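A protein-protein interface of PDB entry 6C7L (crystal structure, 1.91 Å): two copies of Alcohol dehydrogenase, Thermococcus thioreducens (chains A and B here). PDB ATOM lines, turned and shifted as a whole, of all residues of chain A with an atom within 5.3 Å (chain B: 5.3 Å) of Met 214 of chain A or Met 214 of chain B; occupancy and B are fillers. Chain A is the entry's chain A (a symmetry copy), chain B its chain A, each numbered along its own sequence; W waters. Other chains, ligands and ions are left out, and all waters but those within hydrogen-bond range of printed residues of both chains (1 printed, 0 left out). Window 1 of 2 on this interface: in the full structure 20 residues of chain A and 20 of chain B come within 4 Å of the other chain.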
ATOM      1  N   PHE A   2      -5.465  -3.944  -4.437  1.00  0.00           N
ATOM      2  CA  PHE A   2      -6.450  -4.830  -5.063  1.00  0.00           C
ATOM      3  C   PHE A   2      -7.805  -4.587  -4.387  1.00  0.00           C
ATOM      4  O   PHE A   2      -7.909  -4.624  -3.165  1.00  0.00           O
ATOM      5  CB  PHE A   2      -6.013  -6.297  -4.907  1.00  0.00           C
ATOM      6  CG  PHE A   2      -6.940  -7.281  -5.576  1.00  0.00           C
ATOM      7  CD1 PHE A   2      -6.906  -7.472  -6.954  1.00  0.00           C
ATOM      8  CD2 PHE A   2      -7.945  -7.877  -4.865  1.00  0.00           C
ATOM      9  CE1 PHE A   2      -7.827  -8.280  -7.585  1.00  0.00           C
ATOM     10  CE2 PHE A   2      -8.862  -8.706  -5.483  1.00  0.00           C
ATOM     11  CZ  PHE A   2      -8.744  -8.975  -6.837  1.00  0.00           C
ATOM     12  N   PHE A 210      -2.693 -10.601  -6.651  1.00  0.00           N
ATOM     13  CA  PHE A 210      -4.126 -10.771  -6.568  1.00  0.00           C
ATOM     14  C   PHE A 210      -4.767 -10.608  -7.956  1.00  0.00           C
ATOM     15  O   PHE A 210      -5.615 -11.399  -8.351  1.00  0.00           O
ATOM     16  CB  PHE A 210      -4.708  -9.766  -5.536  1.00  0.00           C
ATOM     17  CG  PHE A 210      -4.149  -9.929  -4.161  1.00  0.00           C
ATOM     18  CD1 PHE A 210      -4.594 -10.954  -3.347  1.00  0.00           C
ATOM     19  CD2 PHE A 210      -3.053  -9.204  -3.746  1.00  0.00           C
ATOM     20  CE1 PHE A 210      -4.054 -11.158  -2.086  1.00  0.00           C
ATOM     21  CE2 PHE A 210      -2.454  -9.451  -2.529  1.00  0.00           C
ATOM     22  CZ  PHE A 210      -2.972 -10.416  -1.679  1.00  0.00           C
ATOM     23  N   SER A 211      -4.332  -9.613  -8.722  1.00  0.00           N
ATOM     24  CA  SER A 211      -4.815  -9.474 -10.075  1.00  0.00           C
ATOM     25  C   SER A 211      -4.308 -10.601 -10.968  1.00  0.00           C
ATOM     26  O   SER A 211      -5.032 -11.093 -11.833  1.00  0.00           O
ATOM     27  CB  SER A 211      -4.469  -8.101 -10.668  1.00  0.00           C
ATOM     28  OG  SER A 211      -3.088  -7.850 -10.721  1.00  0.00           O
ATOM     29  N   ASP A 212      -3.087 -11.052 -10.713  1.00  0.00           N
ATOM     30  CA  ASP A 212      -2.489 -12.160 -11.460  1.00  0.00           C
ATOM     31  C   ASP A 212      -3.299 -13.437 -11.301  1.00  0.00           C
ATOM     32  O   ASP A 212      -3.406 -14.249 -12.234  1.00  0.00           O
ATOM     33  CB  ASP A 212      -1.045 -12.412 -10.983  1.00  0.00           C
ATOM     34  CG  ASP A 212      -0.055 -11.306 -11.401  1.00  0.00           C
ATOM     35  OD1 ASP A 212      -0.378 -10.477 -12.287  1.00  0.00           O
ATOM     36  OD2 ASP A 212       1.096 -11.335 -10.892  1.00  0.00           O
ATOM     37  N   ALA A 213      -3.801 -13.677 -10.092  1.00  0.00           N
ATOM     38  CA  ALA A 213      -4.543 -14.905  -9.837  1.00  0.00           C
ATOM     39  C   ALA A 213      -5.723 -14.975 -10.798  1.00  0.00           C
ATOM     40  O   ALA A 213      -6.011 -16.016 -11.357  1.00  0.00           O
ATOM     41  CB  ALA A 213      -5.032 -14.942  -8.406  1.00  0.00           C
ATOM     42  N   MET A 214      -6.423 -13.855 -10.947  1.00  0.00           N
ATOM     43  CA  MET A 214      -7.558 -13.756 -11.856  1.00  0.00           C
ATOM     44  C   MET A 214      -7.118 -13.769 -13.323  1.00  0.00           C
ATOM     45  O   MET A 214      -7.751 -14.435 -14.139  1.00  0.00           O
ATOM     46  CB  MET A 214      -8.351 -12.480 -11.555  1.00  0.00           C
ATOM     47  CG  MET A 214      -9.042 -12.535 -10.219  1.00  0.00           C
ATOM     48  SD  MET A 214     -10.364 -13.766 -10.186  1.00  0.00           S
ATOM     49  CE  MET A 214     -10.821 -13.618  -8.470  1.00  0.00           C
ATOM     50  N   ALA A 215      -6.044 -13.038 -13.662  1.00  0.00           N
ATOM     51  CA  ALA A 215      -5.577 -13.008 -15.049  1.00  0.00           C
ATOM     52  C   ALA A 215      -5.164 -14.398 -15.523  1.00  0.00           C
ATOM     53  O   ALA A 215      -5.569 -14.832 -16.598  1.00  0.00           O
ATOM     54  CB  ALA A 215      -4.430 -12.015 -15.245  1.00  0.00           C
ATOM     55  N   ILE A 216      -4.415 -15.123 -14.689  1.00  0.00           N
ATOM     56  CA  ILE A 216      -3.944 -16.456 -15.081  1.00  0.00           C
ATOM     57  C   ILE A 216      -5.083 -17.430 -15.265  1.00  0.00           C
ATOM     58  O   ILE A 216      -5.126 -18.145 -16.263  1.00  0.00           O
ATOM     59  CB  ILE A 216      -2.923 -17.030 -14.074  1.00  0.00           C
ATOM     60  CG1 ILE A 216      -1.595 -16.326 -14.264  1.00  0.00           C
ATOM     61  CG2 ILE A 216      -2.666 -18.495 -14.340  1.00  0.00           C
ATOM     62  CD1 ILE A 216      -0.953 -16.600 -15.635  1.00  0.00           C
ATOM     63  N   LYS A 217      -6.073 -17.414 -14.359  1.00  0.00           N
ATOM     64  CA  LYS A 217      -7.186 -18.299 -14.569  1.00  0.00           C
ATOM     65  C   LYS A 217      -7.987 -17.995 -15.835  1.00  0.00           C
ATOM     66  O   LYS A 217      -8.385 -18.905 -16.584  1.00  0.00           O
ATOM     67  CB  LYS A 217      -8.075 -18.377 -13.352  1.00  0.00           C
ATOM     68  CG  LYS A 217      -9.120 -19.459 -13.511  1.00  0.00           C
ATOM     69  CD  LYS A 217      -9.403 -20.163 -12.215  1.00  0.00           C
ATOM     70  CE  LYS A 217     -10.645 -21.033 -12.360  1.00  0.00           C
ATOM     71  NZ  LYS A 217     -10.378 -22.248 -13.148  1.00  0.00           N
ATOM     72  N   ALA A 218      -8.196 -16.723 -16.118  1.00  0.00           N
ATOM     73  CA  ALA A 218      -8.897 -16.343 -17.347  1.00  0.00           C
ATOM     74  C   ALA A 218      -8.141 -16.828 -18.614  1.00  0.00           C
ATOM     75  O   ALA A 218      -8.755 -17.326 -19.569  1.00  0.00           O
ATOM     76  CB  ALA A 218      -9.097 -14.852 -17.390  1.00  0.00           C
ATOM     77  N   ILE A 219      -6.835 -16.594 -18.654  1.00  0.00           N
ATOM     78  CA  ILE A 219      -6.008 -16.989 -19.795  1.00  0.00           C
ATOM     79  C   ILE A 219      -6.111 -18.500 -20.062  1.00  0.00           C
ATOM     80  O   ILE A 219      -6.341 -18.925 -21.188  1.00  0.00           O
ATOM     81  CB  ILE A 219      -4.521 -16.618 -19.595  1.00  0.00           C
ATOM     82  CG1 ILE A 219      -4.330 -15.098 -19.646  1.00  0.00           C
ATOM     83  CG2 ILE A 219      -3.662 -17.217 -20.711  1.00  0.00           C
ATOM     84  CD1 ILE A 219      -3.089 -14.614 -18.923  1.00  0.00           C
ATOM     85  N   MET A 246     -13.375 -12.658 -14.785  1.00  0.00           N
ATOM     86  CA  MET A 246     -12.073 -12.792 -14.101  1.00  0.00           C
ATOM     87  C   MET A 246     -11.073 -11.819 -14.687  1.00  0.00           C
ATOM     88  O   MET A 246     -10.333 -11.159 -13.981  1.00  0.00           O
ATOM     89  CB  MET A 246     -11.492 -14.192 -14.294  1.00  0.00           C
ATOM     90  CG  MET A 246     -12.316 -15.297 -13.689  1.00  0.00           C
ATOM     91  SD  MET A 246     -11.554 -16.891 -14.018  1.00  0.00           S
ATOM     92  CE  MET A 246     -12.838 -17.953 -13.352  1.00  0.00           C
ATOM     93  N   ALA A 247     -11.030 -11.769 -16.005  1.00  0.00           N
ATOM     94  CA  ALA A 247     -10.109 -10.873 -16.717  1.00  0.00           C
ATOM     95  C   ALA A 247     -10.470  -9.415 -16.465  1.00  0.00           C
ATOM     96  O   ALA A 247      -9.603  -8.571 -16.309  1.00  0.00           O
ATOM     97  CB  ALA A 247     -10.123 -11.172 -18.208  1.00  0.00           C
ATOM     98  N   ILE A 249     -11.802  -8.396 -13.539  1.00  0.00           N
ATOM     99  CA  ILE A 249     -11.291  -8.149 -12.206  1.00  0.00           C
ATOM    100  C   ILE A 249      -9.797  -7.875 -12.277  1.00  0.00           C
ATOM    101  O   ILE A 249      -9.291  -6.936 -11.640  1.00  0.00           O
ATOM    102  CB  ILE A 249     -11.534  -9.327 -11.239  1.00  0.00           C
ATOM    103  CG1 ILE A 249     -13.046  -9.578 -11.028  1.00  0.00           C
ATOM    104  CG2 ILE A 249     -10.937  -9.006  -9.894  1.00  0.00           C
ATOM    105  CD1 ILE A 249     -13.356 -10.929 -10.387  1.00  0.00           C
ATOM    106  N   ALA A 250      -9.099  -8.623 -13.125  1.00  0.00           N
ATOM    107  CA  ALA A 250      -7.687  -8.394 -13.309  1.00  0.00           C
ATOM    108  C   ALA A 250      -7.385  -6.983 -13.832  1.00  0.00           C
ATOM    109  O   ALA A 250      -6.529  -6.275 -13.265  1.00  0.00           O
ATOM    110  CB  ALA A 250      -7.091  -9.459 -14.207  1.00  0.00           C
ATOM    111  N   PHE B   2     -19.548 -14.322  -5.390  1.00  0.00           N
ATOM    112  CA  PHE B   2     -18.174 -13.937  -5.058  1.00  0.00           C
ATOM    113  C   PHE B   2     -18.168 -12.443  -4.715  1.00  0.00           C
ATOM    114  O   PHE B   2     -18.671 -11.625  -5.480  1.00  0.00           O
ATOM    115  CB  PHE B   2     -17.242 -14.233  -6.247  1.00  0.00           C
ATOM    116  CG  PHE B   2     -15.792 -13.923  -5.973  1.00  0.00           C
ATOM    117  CD1 PHE B   2     -15.008 -14.785  -5.212  1.00  0.00           C
ATOM    118  CD2 PHE B   2     -15.267 -12.708  -6.322  1.00  0.00           C
ATOM    119  CE1 PHE B   2     -13.718 -14.452  -4.860  1.00  0.00           C
ATOM    120  CE2 PHE B   2     -13.968 -12.372  -5.992  1.00  0.00           C
ATOM    121  CZ  PHE B   2     -13.164 -13.289  -5.333  1.00  0.00           C
ATOM    122  N   PHE B 210     -14.256 -18.049  -9.263  1.00  0.00           N
ATOM    123  CA  PHE B 210     -13.614 -16.861  -8.749  1.00  0.00           C
ATOM    124  C   PHE B 210     -12.852 -17.180  -7.454  1.00  0.00           C
ATOM    125  O   PHE B 210     -11.713 -16.764  -7.277  1.00  0.00           O
ATOM    126  CB  PHE B 210     -14.678 -15.747  -8.540  1.00  0.00           C
ATOM    127  CG  PHE B 210     -15.403 -15.370  -9.788  1.00  0.00           C
ATOM    128  CD1 PHE B 210     -14.797 -14.552 -10.724  1.00  0.00           C
ATOM    129  CD2 PHE B 210     -16.593 -15.974 -10.134  1.00  0.00           C
ATOM    130  CE1 PHE B 210     -15.429 -14.230 -11.916  1.00  0.00           C
ATOM    131  CE2 PHE B 210     -17.192 -15.726 -11.350  1.00  0.00           C
ATOM    132  CZ  PHE B 210     -16.623 -14.827 -12.239  1.00  0.00           C
ATOM    133  N   SER B 211     -13.452 -17.962  -6.562  1.00  0.00           N
ATOM    134  CA  SER B 211     -12.747 -18.388  -5.377  1.00  0.00           C
ATOM    135  C   SER B 211     -11.623 -19.361  -5.715  1.00  0.00           C
ATOM    136  O   SER B 211     -10.551 -19.318  -5.113  1.00  0.00           O
ATOM    137  CB  SER B 211     -13.696 -18.983  -4.328  1.00  0.00           C
ATOM    138  OG  SER B 211     -14.397 -20.110  -4.788  1.00  0.00           O
ATOM    139  N   ASP B 212     -11.847 -20.194  -6.723  1.00  0.00           N
ATOM    140  CA  ASP B 212     -10.841 -21.151  -7.187  1.00  0.00           C
ATOM    141  C   ASP B 212      -9.588 -20.444  -7.680  1.00  0.00           C
ATOM    142  O   ASP B 212      -8.464 -20.943  -7.515  1.00  0.00           O
ATOM    143  CB  ASP B 212     -11.413 -22.023  -8.323  1.00  0.00           C
ATOM    144  CG  ASP B 212     -12.476 -23.034  -7.848  1.00  0.00           C
ATOM    145  OD1 ASP B 212     -12.600 -23.287  -6.625  1.00  0.00           O
ATOM    146  OD2 ASP B 212     -13.129 -23.646  -8.734  1.00  0.00           O
ATOM    147  N   ALA B 213      -9.771 -19.322  -8.371  1.00  0.00           N
ATOM    148  CA  ALA B 213      -8.629 -18.610  -8.929  1.00  0.00           C
ATOM    149  C   ALA B 213      -7.674 -18.249  -7.798  1.00  0.00           C
ATOM    150  O   ALA B 213      -6.473 -18.385  -7.928  1.00  0.00           O
ATOM    151  CB  ALA B 213      -9.083 -17.359  -9.648  1.00  0.00           C
ATOM    152  N   MET B 214      -8.232 -17.750  -6.699  1.00  0.00           N
ATOM    153  CA  MET B 214      -7.454 -17.389  -5.521  1.00  0.00           C
ATOM    154  C   MET B 214      -6.925 -18.624  -4.786  1.00  0.00           C
ATOM    155  O   MET B 214      -5.771 -18.629  -4.362  1.00  0.00           O
ATOM    156  CB  MET B 214      -8.311 -16.540  -4.577  1.00  0.00           C
ATOM    157  CG  MET B 214      -8.629 -15.185  -5.151  1.00  0.00           C
ATOM    158  SD  MET B 214      -7.160 -14.145  -5.295  1.00  0.00           S
ATOM    159  CE  MET B 214      -7.906 -12.743  -6.102  1.00  0.00           C
ATOM    160  N   ALA B 215      -7.758 -19.665  -4.628  1.00  0.00           N
ATOM    161  CA  ALA B 215      -7.311 -20.873  -3.931  1.00  0.00           C
ATOM    162  C   ALA B 215      -6.137 -21.525  -4.655  1.00  0.00           C
ATOM    163  O   ALA B 215      -5.134 -21.861  -4.031  1.00  0.00           O
ATOM    164  CB  ALA B 215      -8.448 -21.877  -3.743  1.00  0.00           C
ATOM    165  N   ILE B 216      -6.234 -21.640  -5.981  1.00  0.00           N
ATOM    166  CA  ILE B 216      -5.167 -22.289  -6.750  1.00  0.00           C
ATOM    167  C   ILE B 216      -3.870 -21.517  -6.686  1.00  0.00           C
ATOM    168  O   ILE B 216      -2.816 -22.104  -6.450  1.00  0.00           O
ATOM    169  CB  ILE B 216      -5.568 -22.513  -8.225  1.00  0.00           C
ATOM    170  CG1 ILE B 216      -6.546 -23.667  -8.300  1.00  0.00           C
ATOM    171  CG2 ILE B 216      -4.372 -22.918  -9.056  1.00  0.00           C
ATOM    172  CD1 ILE B 216      -5.930 -25.013  -7.878  1.00  0.00           C
ATOM    173  N   LYS B 217      -3.930 -20.182  -6.799  1.00  0.00           N
ATOM    174  CA  LYS B 217      -2.702 -19.444  -6.676  1.00  0.00           C
ATOM    175  C   LYS B 217      -2.048 -19.559  -5.299  1.00  0.00           C
ATOM    176  O   LYS B 217      -0.820 -19.717  -5.176  1.00  0.00           O
ATOM    177  CB  LYS B 217      -2.871 -18.004  -7.094  1.00  0.00           C
ATOM    178  CG  LYS B 217      -1.535 -17.296  -7.154  1.00  0.00           C
ATOM    179  CD  LYS B 217      -1.473 -16.308  -8.284  1.00  0.00           C
ATOM    180  CE  LYS B 217      -0.238 -15.429  -8.133  1.00  0.00           C
ATOM    181  NZ  LYS B 217       0.999 -16.149  -8.481  1.00  0.00           N
ATOM    182  N   ALA B 218      -2.851 -19.528  -4.252  1.00  0.00           N
ATOM    183  CA  ALA B 218      -2.313 -19.698  -2.900  1.00  0.00           C
ATOM    184  C   ALA B 218      -1.620 -21.078  -2.726  1.00  0.00           C
ATOM    185  O   ALA B 218      -0.543 -21.177  -2.121  1.00  0.00           O
ATOM    186  CB  ALA B 218      -3.406 -19.524  -1.881  1.00  0.00           C
ATOM    187  N   ILE B 219      -2.285 -22.138  -3.169  1.00  0.00           N
ATOM    188  CA  ILE B 219      -1.751 -23.496  -3.057  1.00  0.00           C
ATOM    189  C   ILE B 219      -0.382 -23.616  -3.746  1.00  0.00           C
ATOM    190  O   ILE B 219       0.572 -24.121  -3.165  1.00  0.00           O
ATOM    191  CB  ILE B 219      -2.706 -24.552  -3.658  1.00  0.00           C
ATOM    192  CG1 ILE B 219      -3.968 -24.693  -2.799  1.00  0.00           C
ATOM    193  CG2 ILE B 219      -2.033 -25.925  -3.698  1.00  0.00           C
ATOM    194  CD1 ILE B 219      -5.165 -25.235  -3.555  1.00  0.00           C
ATOM    195  N   MET B 246      -4.747 -14.482  -0.244  1.00  0.00           N
ATOM    196  CA  MET B 246      -5.455 -15.113  -1.376  1.00  0.00           C
ATOM    197  C   MET B 246      -6.338 -16.236  -0.879  1.00  0.00           C
ATOM    198  O   MET B 246      -7.476 -16.384  -1.284  1.00  0.00           O
ATOM    199  CB  MET B 246      -4.469 -15.731  -2.366  1.00  0.00           C
ATOM    200  CG  MET B 246      -3.557 -14.739  -3.037  1.00  0.00           C
ATOM    201  SD  MET B 246      -2.421 -15.589  -4.142  1.00  0.00           S
ATOM    202  CE  MET B 246      -1.397 -14.193  -4.611  1.00  0.00           C
ATOM    203  N   ALA B 247      -5.777 -17.063  -0.016  1.00  0.00           N
ATOM    204  CA  ALA B 247      -6.510 -18.202   0.553  1.00  0.00           C
ATOM    205  C   ALA B 247      -7.654 -17.723   1.437  1.00  0.00           C
ATOM    206  O   ALA B 247      -8.730 -18.297   1.439  1.00  0.00           O
ATOM    207  CB  ALA B 247      -5.569 -19.097   1.345  1.00  0.00           C
ATOM    208  N   ILE B 249      -9.328 -14.869   0.781  1.00  0.00           N
ATOM    209  CA  ILE B 249     -10.344 -14.468  -0.171  1.00  0.00           C
ATOM    210  C   ILE B 249     -11.097 -15.695  -0.659  1.00  0.00           C
ATOM    211  O   ILE B 249     -12.336 -15.690  -0.743  1.00  0.00           O
ATOM    212  CB  ILE B 249      -9.763 -13.725  -1.393  1.00  0.00           C
ATOM    213  CG1 ILE B 249      -9.087 -12.397  -0.973  1.00  0.00           C
ATOM    214  CG2 ILE B 249     -10.876 -13.381  -2.349  1.00  0.00           C
ATOM    215  CD1 ILE B 249      -8.191 -11.801  -2.056  1.00  0.00           C
ATOM    216  N   ALA B 250     -10.369 -16.783  -0.888  1.00  0.00           N
ATOM    217  CA  ALA B 250     -11.003 -18.014  -1.291  1.00  0.00           C
ATOM    218  C   ALA B 250     -11.999 -18.532  -0.244  1.00  0.00           C
ATOM    219  O   ALA B 250     -13.155 -18.854  -0.585  1.00  0.00           O
ATOM    220  CB  ALA B 250      -9.961 -19.060  -1.630  1.00  0.00           C
HETATM  221  O   HOH W   1      -5.259 -18.466 -10.384  1.00  0.00           O
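Phe 210 of chain A touches Met 246 of chain B, and with the chains exchanged Met 246 of chain A touches Phe 210 of chain B.
Ala 213 of chain A touches Met 214 of chain B, and with the chains exchanged Met 214 of chain A touches Ala 213 of chain B.
Ala 213 of chain A touches Lys 217 of chain B, and with the chains exchanged Lys 217 of chain A touches Ala 213 of chain B.
Met 214 of chain B touches its own counterpart, Met 214 of chain A.
Positions printed for both chains: 2, 210, 211, 212, 213, 214, 215, 216, 217, 218, 219, 246, 247, 249 and 250.
Of the 14 pairs that touch across the chains among the printed residues, 14 have their exchanged pair printed and touching as well.
Met 214 of chain A touches four residues of chain B.
Met 214 of chain B touches just these residues of chain A: Phe 2, Phe 210, Ala 213 and Met 214.
Printed residues of chain B within 4 Å of Ala 213 of chain A: Ala 213 (3.8 Å), Met 214 (3.9 Å) and Lys 217 (3.7 Å).
Of the printed residues of chain A, Phe 210 of chain B touches Met 214, Met 246 and Ile 249.
The nearest printed residue of chain B that does not touch Met 214 of chain A is Ser 211 of chain B (5.4 Å).
The nearest printed residue of chain A that does not touch Lys 217 of chain B is Asp 212 of chain A (4.2 Å).
Among the printed residues, pairs that only touch across the chains: Phe 2 of chain A with Met 214 of chain B, Phe 210 of chain A with Met 214 of chain B, Phe 210 of chain A with Met 246 of chain B, Phe 210 of chain A with Ile 249 of chain B, Ala 213 of chain A with Ala 213 of chain B, Ala 213 of chain A with Met 214 of chain B, Ala 213 of chain A with Lys 217 of chain B, Met 214 of chain A with Phe 2 of chain B, Met 214 of chain A with Phe 210 of chain B, Met 214 of chain A with Ala 213 of chain B, Met 214 of chain A with Met 214 of chain B, Lys 217 of chain A with Ala 213 of chain B, Met 246 of chain A with Phe 210 of chain B and Ile 249 of chain A with Phe 210 of chain B.
Of the 15 printed residues of chain B, 7 touch a printed residue of chain A.
Hydrophobic or aromatic side chains of chain B within 4 Å of the printed part of chain A: Phe 2, Phe 210, Ala 213, Met 214, Met 246 and Ile 249.
Printed residues of chain A that touch a printed residue of chain B: Phe 2, Phe 210, Ala 213, Met 214, Lys 217, Met 246 and Ile 249.
Hydrophobic or aromatic side chains of chain A within 4 Å of the printed part of chain B: Phe 2, Phe 210, Ala 213, Met 214, Met 246 and Ile 249.
Among the printed residues, 14 pairs touch across the chains.
Among the printed residues, no Asp or Glu carboxylate lies within 4 Å of a Lys or Arg side-chain nitrogen of the other chain.
Water W1 bridges O of Ala 213 of chain B (2.7 Å) and O of Ala 213 of chain A (2.7 Å).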
